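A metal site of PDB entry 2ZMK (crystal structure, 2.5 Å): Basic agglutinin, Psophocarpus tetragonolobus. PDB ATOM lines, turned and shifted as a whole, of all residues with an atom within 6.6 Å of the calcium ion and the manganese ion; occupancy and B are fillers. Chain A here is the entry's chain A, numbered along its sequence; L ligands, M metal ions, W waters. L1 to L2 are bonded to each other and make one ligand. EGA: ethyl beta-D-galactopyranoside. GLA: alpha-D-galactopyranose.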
ATOM      1  N   ASP A  87      10.912 -26.357  -1.472  1.00  0.00           N
ATOM      2  CA  ASP A  87      12.187 -26.282  -2.176  1.00  0.00           C
ATOM      3  C   ASP A  87      13.300 -25.723  -1.285  1.00  0.00           C
ATOM      4  O   ASP A  87      14.485 -26.007  -1.503  1.00  0.00           O
ATOM      5  CB  ASP A  87      12.051 -25.412  -3.415  1.00  0.00           C
ATOM      6  CG  ASP A  87      11.667 -26.211  -4.645  1.00  0.00           C
ATOM      7  OD1 ASP A  87      10.456 -26.419  -4.864  1.00  0.00           O
ATOM      8  OD2 ASP A  87      12.571 -26.649  -5.381  1.00  0.00           O
ATOM      9  N   GLY A 104       9.376 -22.591  -6.979  1.00  0.00           N
ATOM     10  CA  GLY A 104      10.157 -23.794  -7.124  1.00  0.00           C
ATOM     11  C   GLY A 104      11.618 -23.632  -6.733  1.00  0.00           C
ATOM     12  O   GLY A 104      11.944 -22.974  -5.732  1.00  0.00           O
ATOM     13  N   GLY A 105      12.508 -24.220  -7.517  1.00  0.00           N
ATOM     14  CA  GLY A 105      13.925 -24.150  -7.245  1.00  0.00           C
ATOM     15  C   GLY A 105      14.522 -22.765  -7.342  1.00  0.00           C
ATOM     16  O   GLY A 105      15.710 -22.580  -7.067  1.00  0.00           O
ATOM     17  N   TYR A 106      13.722 -21.782  -7.731  1.00  0.00           N
ATOM     18  CA  TYR A 106      14.208 -20.409  -7.828  1.00  0.00           C
ATOM     19  C   TYR A 106      13.873 -19.598  -6.573  1.00  0.00           C
ATOM     20  O   TYR A 106      14.181 -18.407  -6.487  1.00  0.00           O
ATOM     21  CB  TYR A 106      13.645 -19.723  -9.071  1.00  0.00           C
ATOM     22  CG  TYR A 106      14.130 -20.353 -10.347  1.00  0.00           C
ATOM     23  CD1 TYR A 106      15.489 -20.401 -10.651  1.00  0.00           C
ATOM     24  CD2 TYR A 106      13.234 -20.909 -11.249  1.00  0.00           C
ATOM     25  CE1 TYR A 106      15.950 -20.997 -11.821  1.00  0.00           C
ATOM     26  CE2 TYR A 106      13.681 -21.514 -12.435  1.00  0.00           C
ATOM     27  CZ  TYR A 106      15.046 -21.558 -12.708  1.00  0.00           C
ATOM     28  OH  TYR A 106      15.482 -22.163 -13.866  1.00  0.00           O
ATOM     29  N   PHE A 107      13.236 -20.261  -5.619  1.00  0.00           N
ATOM     30  CA  PHE A 107      12.898 -19.667  -4.320  1.00  0.00           C
ATOM     31  C   PHE A 107      12.082 -18.378  -4.354  1.00  0.00           C
ATOM     32  O   PHE A 107      11.809 -17.809  -3.306  1.00  0.00           O
ATOM     33  CB  PHE A 107      14.183 -19.407  -3.538  1.00  0.00           C
ATOM     34  CG  PHE A 107      15.133 -20.568  -3.498  1.00  0.00           C
ATOM     35  CD1 PHE A 107      14.800 -21.730  -2.801  1.00  0.00           C
ATOM     36  CD2 PHE A 107      16.376 -20.486  -4.128  1.00  0.00           C
ATOM     37  CE1 PHE A 107      15.703 -22.804  -2.731  1.00  0.00           C
ATOM     38  CE2 PHE A 107      17.270 -21.546  -4.064  1.00  0.00           C
ATOM     39  CZ  PHE A 107      16.938 -22.708  -3.367  1.00  0.00           C
ATOM     40  N   GLU A 122      21.176 -19.508   0.619  1.00  0.00           N
ATOM     41  CA  GLU A 122      20.081 -20.453   0.529  1.00  0.00           C
ATOM     42  C   GLU A 122      20.243 -21.681   1.393  1.00  0.00           C
ATOM     43  O   GLU A 122      21.356 -22.108   1.712  1.00  0.00           O
ATOM     44  CB  GLU A 122      19.924 -20.931  -0.922  1.00  0.00           C
ATOM     45  CG  GLU A 122      21.153 -21.665  -1.406  1.00  0.00           C
ATOM     46  CD  GLU A 122      20.974 -22.307  -2.766  1.00  0.00           C
ATOM     47  OE1 GLU A 122      20.646 -21.594  -3.734  1.00  0.00           O
ATOM     48  OE2 GLU A 122      21.168 -23.532  -2.844  1.00  0.00           O
ATOM     49  N   ASP A 124      18.829 -24.973   0.742  1.00  0.00           N
ATOM     50  CA  ASP A 124      18.235 -25.777  -0.300  1.00  0.00           C
ATOM     51  C   ASP A 124      17.869 -27.181   0.116  1.00  0.00           C
ATOM     52  O   ASP A 124      18.718 -27.933   0.596  1.00  0.00           O
ATOM     53  CB  ASP A 124      19.188 -25.838  -1.477  1.00  0.00           C
ATOM     54  CG  ASP A 124      18.466 -26.002  -2.772  1.00  0.00           C
ATOM     55  OD1 ASP A 124      17.410 -26.666  -2.774  1.00  0.00           O
ATOM     56  OD2 ASP A 124      18.951 -25.455  -3.779  1.00  0.00           O
ATOM     57  N   THR A 125      16.617 -27.553  -0.115  1.00  0.00           N
ATOM     58  CA  THR A 125      16.137 -28.857   0.288  1.00  0.00           C
ATOM     59  C   THR A 125      15.759 -29.811  -0.853  1.00  0.00           C
ATOM     60  O   THR A 125      15.545 -30.997  -0.615  1.00  0.00           O
ATOM     61  CB  THR A 125      14.915 -28.701   1.205  1.00  0.00           C
ATOM     62  OG1 THR A 125      13.902 -27.952   0.527  1.00  0.00           O
ATOM     63  CG2 THR A 125      15.309 -27.981   2.469  1.00  0.00           C
ATOM     64  N   PHE A 126      15.684 -29.299  -2.080  1.00  0.00           N
ATOM     65  CA  PHE A 126      15.345 -30.125  -3.222  1.00  0.00           C
ATOM     66  C   PHE A 126      16.485 -30.108  -4.220  1.00  0.00           C
ATOM     67  O   PHE A 126      17.020 -29.053  -4.532  1.00  0.00           O
ATOM     68  CB  PHE A 126      14.092 -29.587  -3.912  1.00  0.00           C
ATOM     69  CG  PHE A 126      13.707 -30.369  -5.117  1.00  0.00           C
ATOM     70  CD1 PHE A 126      13.130 -31.631  -4.978  1.00  0.00           C
ATOM     71  CD2 PHE A 126      13.943 -29.874  -6.394  1.00  0.00           C
ATOM     72  CE1 PHE A 126      12.796 -32.387  -6.095  1.00  0.00           C
ATOM     73  CE2 PHE A 126      13.609 -30.621  -7.522  1.00  0.00           C
ATOM     74  CZ  PHE A 126      13.037 -31.884  -7.373  1.00  0.00           C
ATOM     75  N   ARG A 127      16.855 -31.272  -4.748  1.00  0.00           N
ATOM     76  CA  ARG A 127      17.955 -31.304  -5.695  1.00  0.00           C
ATOM     77  C   ARG A 127      17.569 -31.090  -7.151  1.00  0.00           C
ATOM     78  O   ARG A 127      17.059 -31.998  -7.814  1.00  0.00           O
ATOM     79  CB  ARG A 127      18.731 -32.621  -5.563  1.00  0.00           C
ATOM     80  CG  ARG A 127      19.952 -32.658  -6.449  1.00  0.00           C
ATOM     81  CD  ARG A 127      20.833 -33.851  -6.172  1.00  0.00           C
ATOM     82  NE  ARG A 127      22.085 -33.764  -6.930  1.00  0.00           N
ATOM     83  CZ  ARG A 127      23.082 -34.639  -6.817  1.00  0.00           C
ATOM     84  NH1 ARG A 127      22.977 -35.660  -5.982  1.00  0.00           N
ATOM     85  NH2 ARG A 127      24.187 -34.483  -7.540  1.00  0.00           N
ATOM     86  N   ASN A 128      17.825 -29.887  -7.658  1.00  0.00           N
ATOM     87  CA  ASN A 128      17.546 -29.577  -9.051  1.00  0.00           C
ATOM     88  C   ASN A 128      18.742 -30.064  -9.863  1.00  0.00           C
ATOM     89  O   ASN A 128      19.719 -30.556  -9.297  1.00  0.00           O
ATOM     90  CB  ASN A 128      17.356 -28.068  -9.250  1.00  0.00           C
ATOM     91  CG  ASN A 128      16.019 -27.591  -8.727  1.00  0.00           C
ATOM     92  OD1 ASN A 128      15.791 -27.558  -7.522  1.00  0.00           O
ATOM     93  ND2 ASN A 128      15.108 -27.245  -9.641  1.00  0.00           N
ATOM     94  N   TRP A 130      21.004 -28.409 -11.340  1.00  0.00           N
ATOM     95  CA  TRP A 130      22.198 -27.611 -11.052  1.00  0.00           C
ATOM     96  C   TRP A 130      22.698 -27.737  -9.604  1.00  0.00           C
ATOM     97  O   TRP A 130      23.648 -27.056  -9.207  1.00  0.00           O
ATOM     98  CB  TRP A 130      21.890 -26.141 -11.350  1.00  0.00           C
ATOM     99  CG  TRP A 130      20.750 -25.613 -10.530  1.00  0.00           C
ATOM    100  CD1 TRP A 130      20.772 -25.307  -9.201  1.00  0.00           C
ATOM    101  CD2 TRP A 130      19.415 -25.394 -10.973  1.00  0.00           C
ATOM    102  NE1 TRP A 130      19.527 -24.897  -8.786  1.00  0.00           N
ATOM    103  CE2 TRP A 130      18.670 -24.938  -9.855  1.00  0.00           C
ATOM    104  CE3 TRP A 130      18.752 -25.520 -12.205  1.00  0.00           C
ATOM    105  CZ2 TRP A 130      17.317 -24.616  -9.932  1.00  0.00           C
ATOM    106  CZ3 TRP A 130      17.399 -25.198 -12.282  1.00  0.00           C
ATOM    107  CH2 TRP A 130      16.695 -24.749 -11.153  1.00  0.00           C
ATOM    108  N   ASP A 131      22.060 -28.617  -8.832  1.00  0.00           N
ATOM    109  CA  ASP A 131      22.408 -28.800  -7.432  1.00  0.00           C
ATOM    110  C   ASP A 131      23.208 -30.012  -7.046  1.00  0.00           C
ATOM    111  O   ASP A 131      23.163 -31.041  -7.722  1.00  0.00           O
ATOM    112  CB  ASP A 131      21.150 -28.905  -6.548  1.00  0.00           C
ATOM    113  CG  ASP A 131      20.461 -27.597  -6.330  1.00  0.00           C
ATOM    114  OD1 ASP A 131      21.157 -26.569  -6.140  1.00  0.00           O
ATOM    115  OD2 ASP A 131      19.224 -27.612  -6.320  1.00  0.00           O
ATOM    116  N   PRO A 132      23.964 -29.904  -5.954  1.00  0.00           N
ATOM    117  CA  PRO A 132      24.780 -30.991  -5.421  1.00  0.00           C
ATOM    118  C   PRO A 132      23.827 -31.645  -4.414  1.00  0.00           C
ATOM    119  O   PRO A 132      22.663 -31.262  -4.337  1.00  0.00           O
ATOM    120  CB  PRO A 132      25.933 -30.256  -4.743  1.00  0.00           C
ATOM    121  CG  PRO A 132      25.290 -29.009  -4.260  1.00  0.00           C
ATOM    122  CD  PRO A 132      24.447 -28.603  -5.443  1.00  0.00           C
ATOM    123  N   ILE A 134      21.505 -32.672  -1.341  1.00  0.00           N
ATOM    124  CA  ILE A 134      20.701 -31.818  -0.484  1.00  0.00           C
ATOM    125  C   ILE A 134      20.453 -32.546   0.841  1.00  0.00           C
ATOM    126  O   ILE A 134      20.537 -33.768   0.909  1.00  0.00           O
ATOM    127  CB  ILE A 134      19.333 -31.410  -1.146  1.00  0.00           C
ATOM    128  CG1 ILE A 134      18.582 -32.638  -1.681  1.00  0.00           C
ATOM    129  CG2 ILE A 134      19.575 -30.420  -2.258  1.00  0.00           C
ATOM    130  CD1 ILE A 134      17.882 -33.486  -0.615  1.00  0.00           C
ATOM    131  N   HIS A 136      21.543 -28.451   1.521  1.00  0.00           N
ATOM    132  CA  HIS A 136      22.832 -27.781   1.514  1.00  0.00           C
ATOM    133  C   HIS A 136      22.680 -26.278   1.668  1.00  0.00           C
ATOM    134  O   HIS A 136      21.630 -25.715   1.336  1.00  0.00           O
ATOM    135  CB  HIS A 136      23.615 -28.094   0.239  1.00  0.00           C
ATOM    136  CG  HIS A 136      22.943 -27.666  -1.032  1.00  0.00           C
ATOM    137  ND1 HIS A 136      22.412 -28.573  -1.921  1.00  0.00           N
ATOM    138  CD2 HIS A 136      22.737 -26.439  -1.557  1.00  0.00           C
ATOM    139  CE1 HIS A 136      21.909 -27.912  -2.960  1.00  0.00           C
ATOM    140  NE2 HIS A 136      22.098 -26.616  -2.760  1.00  0.00           N
ATOM    141  N   ILE A 137      23.706 -25.652   2.213  1.00  0.00           N
ATOM    142  CA  ILE A 137      23.719 -24.198   2.368  1.00  0.00           C
ATOM    143  C   ILE A 137      24.430 -23.755   1.112  1.00  0.00           C
ATOM    144  O   ILE A 137      25.369 -24.417   0.660  1.00  0.00           O
ATOM    145  CB  ILE A 137      24.564 -23.730   3.551  1.00  0.00           C
ATOM    146  CG1 ILE A 137      24.133 -24.434   4.825  1.00  0.00           C
ATOM    147  CG2 ILE A 137      24.408 -22.245   3.717  1.00  0.00           C
ATOM    148  CD1 ILE A 137      25.008 -24.103   6.028  1.00  0.00           C
ATOM    149  N   GLY A 138      23.996 -22.653   0.528  1.00  0.00           N
ATOM    150  CA  GLY A 138      24.647 -22.179  -0.660  1.00  0.00           C
ATOM    151  C   GLY A 138      24.746 -20.677  -0.683  1.00  0.00           C
ATOM    152  O   GLY A 138      23.918 -19.980  -0.116  1.00  0.00           O
ATOM    153  N   ASP A 140      24.624 -17.633  -3.132  1.00  0.00           N
ATOM    154  CA  ASP A 140      24.161 -17.289  -4.472  1.00  0.00           C
ATOM    155  C   ASP A 140      24.387 -15.843  -4.858  1.00  0.00           C
ATOM    156  O   ASP A 140      24.051 -14.927  -4.115  1.00  0.00           O
ATOM    157  CB  ASP A 140      22.667 -17.593  -4.629  1.00  0.00           C
ATOM    158  CG  ASP A 140      22.313 -19.027  -4.278  1.00  0.00           C
ATOM    159  OD1 ASP A 140      23.211 -19.889  -4.237  1.00  0.00           O
ATOM    160  OD2 ASP A 140      21.115 -19.289  -4.044  1.00  0.00           O
ATOM    161  N   VAL A 144      20.884 -18.955  -8.949  1.00  0.00           N
ATOM    162  CA  VAL A 144      20.602 -20.029  -8.025  1.00  0.00           C
ATOM    163  C   VAL A 144      21.687 -21.102  -8.118  1.00  0.00           C
ATOM    164  O   VAL A 144      21.684 -22.063  -7.354  1.00  0.00           O
ATOM    165  CB  VAL A 144      19.192 -20.609  -8.334  1.00  0.00           C
ATOM    166  CG1 VAL A 144      19.015 -21.951  -7.696  1.00  0.00           C
ATOM    167  CG2 VAL A 144      18.137 -19.645  -7.790  1.00  0.00           C
ATOM    168  N   ILE A 145      22.612 -20.942  -9.052  1.00  0.00           N
ATOM    169  CA  ILE A 145      23.711 -21.899  -9.154  1.00  0.00           C
ATOM    170  C   ILE A 145      24.785 -21.357  -8.222  1.00  0.00           C
ATOM    171  O   ILE A 145      25.592 -20.518  -8.599  1.00  0.00           O
ATOM    172  CB  ILE A 145      24.249 -21.987 -10.603  1.00  0.00           C
ATOM    173  CG1 ILE A 145      23.139 -22.509 -11.527  1.00  0.00           C
ATOM    174  CG2 ILE A 145      25.436 -22.945 -10.662  1.00  0.00           C
ATOM    175  CD1 ILE A 145      23.543 -22.554 -12.983  1.00  0.00           C
ATOM    176  N   SER A 146      24.783 -21.853  -6.988  1.00  0.00           N
ATOM    177  CA  SER A 146      25.704 -21.406  -5.948  1.00  0.00           C
ATOM    178  C   SER A 146      27.177 -21.376  -6.318  1.00  0.00           C
ATOM    179  O   SER A 146      27.648 -22.204  -7.079  1.00  0.00           O
ATOM    180  CB  SER A 146      25.524 -22.287  -4.703  1.00  0.00           C
ATOM    181  OG  SER A 146      24.171 -22.358  -4.354  1.00  0.00           O
ATOM    182  N   THR A 149      29.072 -24.306  -1.825  1.00  0.00           N
ATOM    183  CA  THR A 149      28.033 -25.153  -1.271  1.00  0.00           C
ATOM    184  C   THR A 149      28.581 -26.013  -0.144  1.00  0.00           C
ATOM    185  O   THR A 149      29.758 -26.338  -0.123  1.00  0.00           O
ATOM    186  CB  THR A 149      27.482 -26.073  -2.388  1.00  0.00           C
ATOM    187  OG1 THR A 149      26.174 -25.639  -2.763  1.00  0.00           O
ATOM    188  CG2 THR A 149      27.447 -27.536  -1.945  1.00  0.00           C
HETATM  189  C2  EGA L   1      12.069 -32.327 -11.471  1.00  0.00           C
HETATM  190  C3  EGA L   1      10.546 -32.219 -11.225  1.00  0.00           C
HETATM  191  C4  EGA L   1      10.071 -30.826 -11.644  1.00  0.00           C
HETATM  192  O5  EGA L   1      11.861 -30.692 -13.279  1.00  0.00           O
HETATM  193  C7  EGA L   1      14.332 -31.758 -14.430  1.00  0.00           C
HETATM  194  C8  EGA L   1      15.163 -32.957 -14.884  1.00  0.00           C
HETATM  195  C1  EGA L   1      12.368 -32.003 -12.938  1.00  0.00           C
HETATM  196  C5  EGA L   1      10.426 -30.599 -13.113  1.00  0.00           C
HETATM  197  C6  EGA L   1       9.961 -29.230 -13.629  1.00  0.00           C
HETATM  198  O1  EGA L   1      13.736 -32.041 -13.167  1.00  0.00           O
HETATM  199  O2  EGA L   1      12.525 -33.630 -11.161  1.00  0.00           O
HETATM  200  O3  EGA L   1      10.238 -32.445  -9.860  1.00  0.00           O
HETATM  201  O4  EGA L   1      10.734 -29.829 -10.830  1.00  0.00           O
HETATM  202  O6  EGA L   1      10.975 -28.566 -14.374  1.00  0.00           O
HETATM  203  C1  GLA L   2       9.910 -28.863 -10.270  1.00  0.00           C
HETATM  204  C2  GLA L   2      10.764 -27.690  -9.747  1.00  0.00           C
HETATM  205  C3  GLA L   2      11.605 -28.159  -8.544  1.00  0.00           C
HETATM  206  C4  GLA L   2      10.680 -28.736  -7.479  1.00  0.00           C
HETATM  207  C5  GLA L   2       9.871 -29.891  -8.081  1.00  0.00           C
HETATM  208  C6  GLA L   2       8.890 -30.502  -7.102  1.00  0.00           C
HETATM  209  O2  GLA L   2      11.620 -27.209 -10.783  1.00  0.00           O
HETATM  210  O3  GLA L   2      12.342 -27.061  -8.009  1.00  0.00           O
HETATM  211  O4  GLA L   2       9.791 -27.732  -7.008  1.00  0.00           O
HETATM  212  O5  GLA L   2       9.109 -29.401  -9.211  1.00  0.00           O
HETATM  213  O6  GLA L   2       8.237 -31.626  -7.670  1.00  0.00           O
HETATM  214 CA    CA M   1      17.099 -26.678  -5.311  1.00  0.00          CA
HETATM  215 MN    MN M   2      21.207 -25.302  -4.300  1.00  0.00          MN
HETATM  216  O   HOH W   1      20.305 -23.672  -5.532  1.00  0.00           O
HETATM  217  O   HOH W   2      14.667 -25.593  -4.484  1.00  0.00           O
HETATM  218  O   HOH W   3      23.186 -24.432  -5.172  1.00  0.00           O
HETATM  219  O   HOH W   4      17.703 -24.239  -6.383  1.00  0.00           O
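The backbone carbonyl oxygen (O) of Asp 131 is in hydrogen-bond range of the guanidinium group (NE) of Arg 127 (3.0 Å).
The backbone carbonyl oxygen (O) of Gly 138 is in hydrogen-bond range of the backbone NH (N) of Glu 122 (2.9 Å).
Four residues have an atom within 4 Å of the calcium ion: Asp 124, Phe 126, Asn 128 and Asp 131.
The nearest printed residue that does not touch the calcium ion is Phe 107 (4.4 Å).
The manganese ion is bound by a ring nitrogen (NE2) of His 136 (2.2 Å), water W1 (2.2 Å), the side-chain carboxylate of Asp 131 (2.2 Å), the side-chain carboxylate of Glu 122 (2.3 Å), the side-chain carboxylate of Asp 124 (2.3 Å) and water W3 (2.3 Å).
The manganese ion has six donor atoms within binding distance.
Water W4 lies within hydrogen-bond range of the backbone carbonyl oxygen of Gly 105 (2.7 Å) and the indole nitrogen of Trp 130 (3.1 Å).
Water W1 lies within hydrogen-bond range of OE1 of Glu 122 (2.8 Å) and O of Val 144 (2.8 Å).
The calcium ion is bound by O of Phe 126, at 2.5 Å.
The calcium ion is bound by the side-chain carboxylate (OD2) of Asp 131, 2.5 Å away.
OD1 of Asp 124 binds the calcium ion, at 2.6 Å.
OD2 of Asp 124 binds the calcium ion.
OD1 of Asn 128 binds the calcium ion, 2.7 Å away.
The calcium ion is bound by water W4 (2.7 Å).
Water W2 binds the calcium ion (2.8 Å).
Four residues have an atom within 4 Å of the manganese ion: Glu 122, Asp 124, Asp 131 and His 136.
An oxygen (O3) of GLA L2 is in hydrogen-bond range of the backbone NH of Gly 105 (2.9 Å).
The side-chain carboxylate of Asp 87 lies within hydrogen-bond range of an oxygen (O4) of GLA L2, at 2.6 Å.
The side-chain amide nitrogen (ND2) of Asn 128 is in hydrogen-bond range of an oxygen (O3) of GLA L2, 3.2 Å away.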
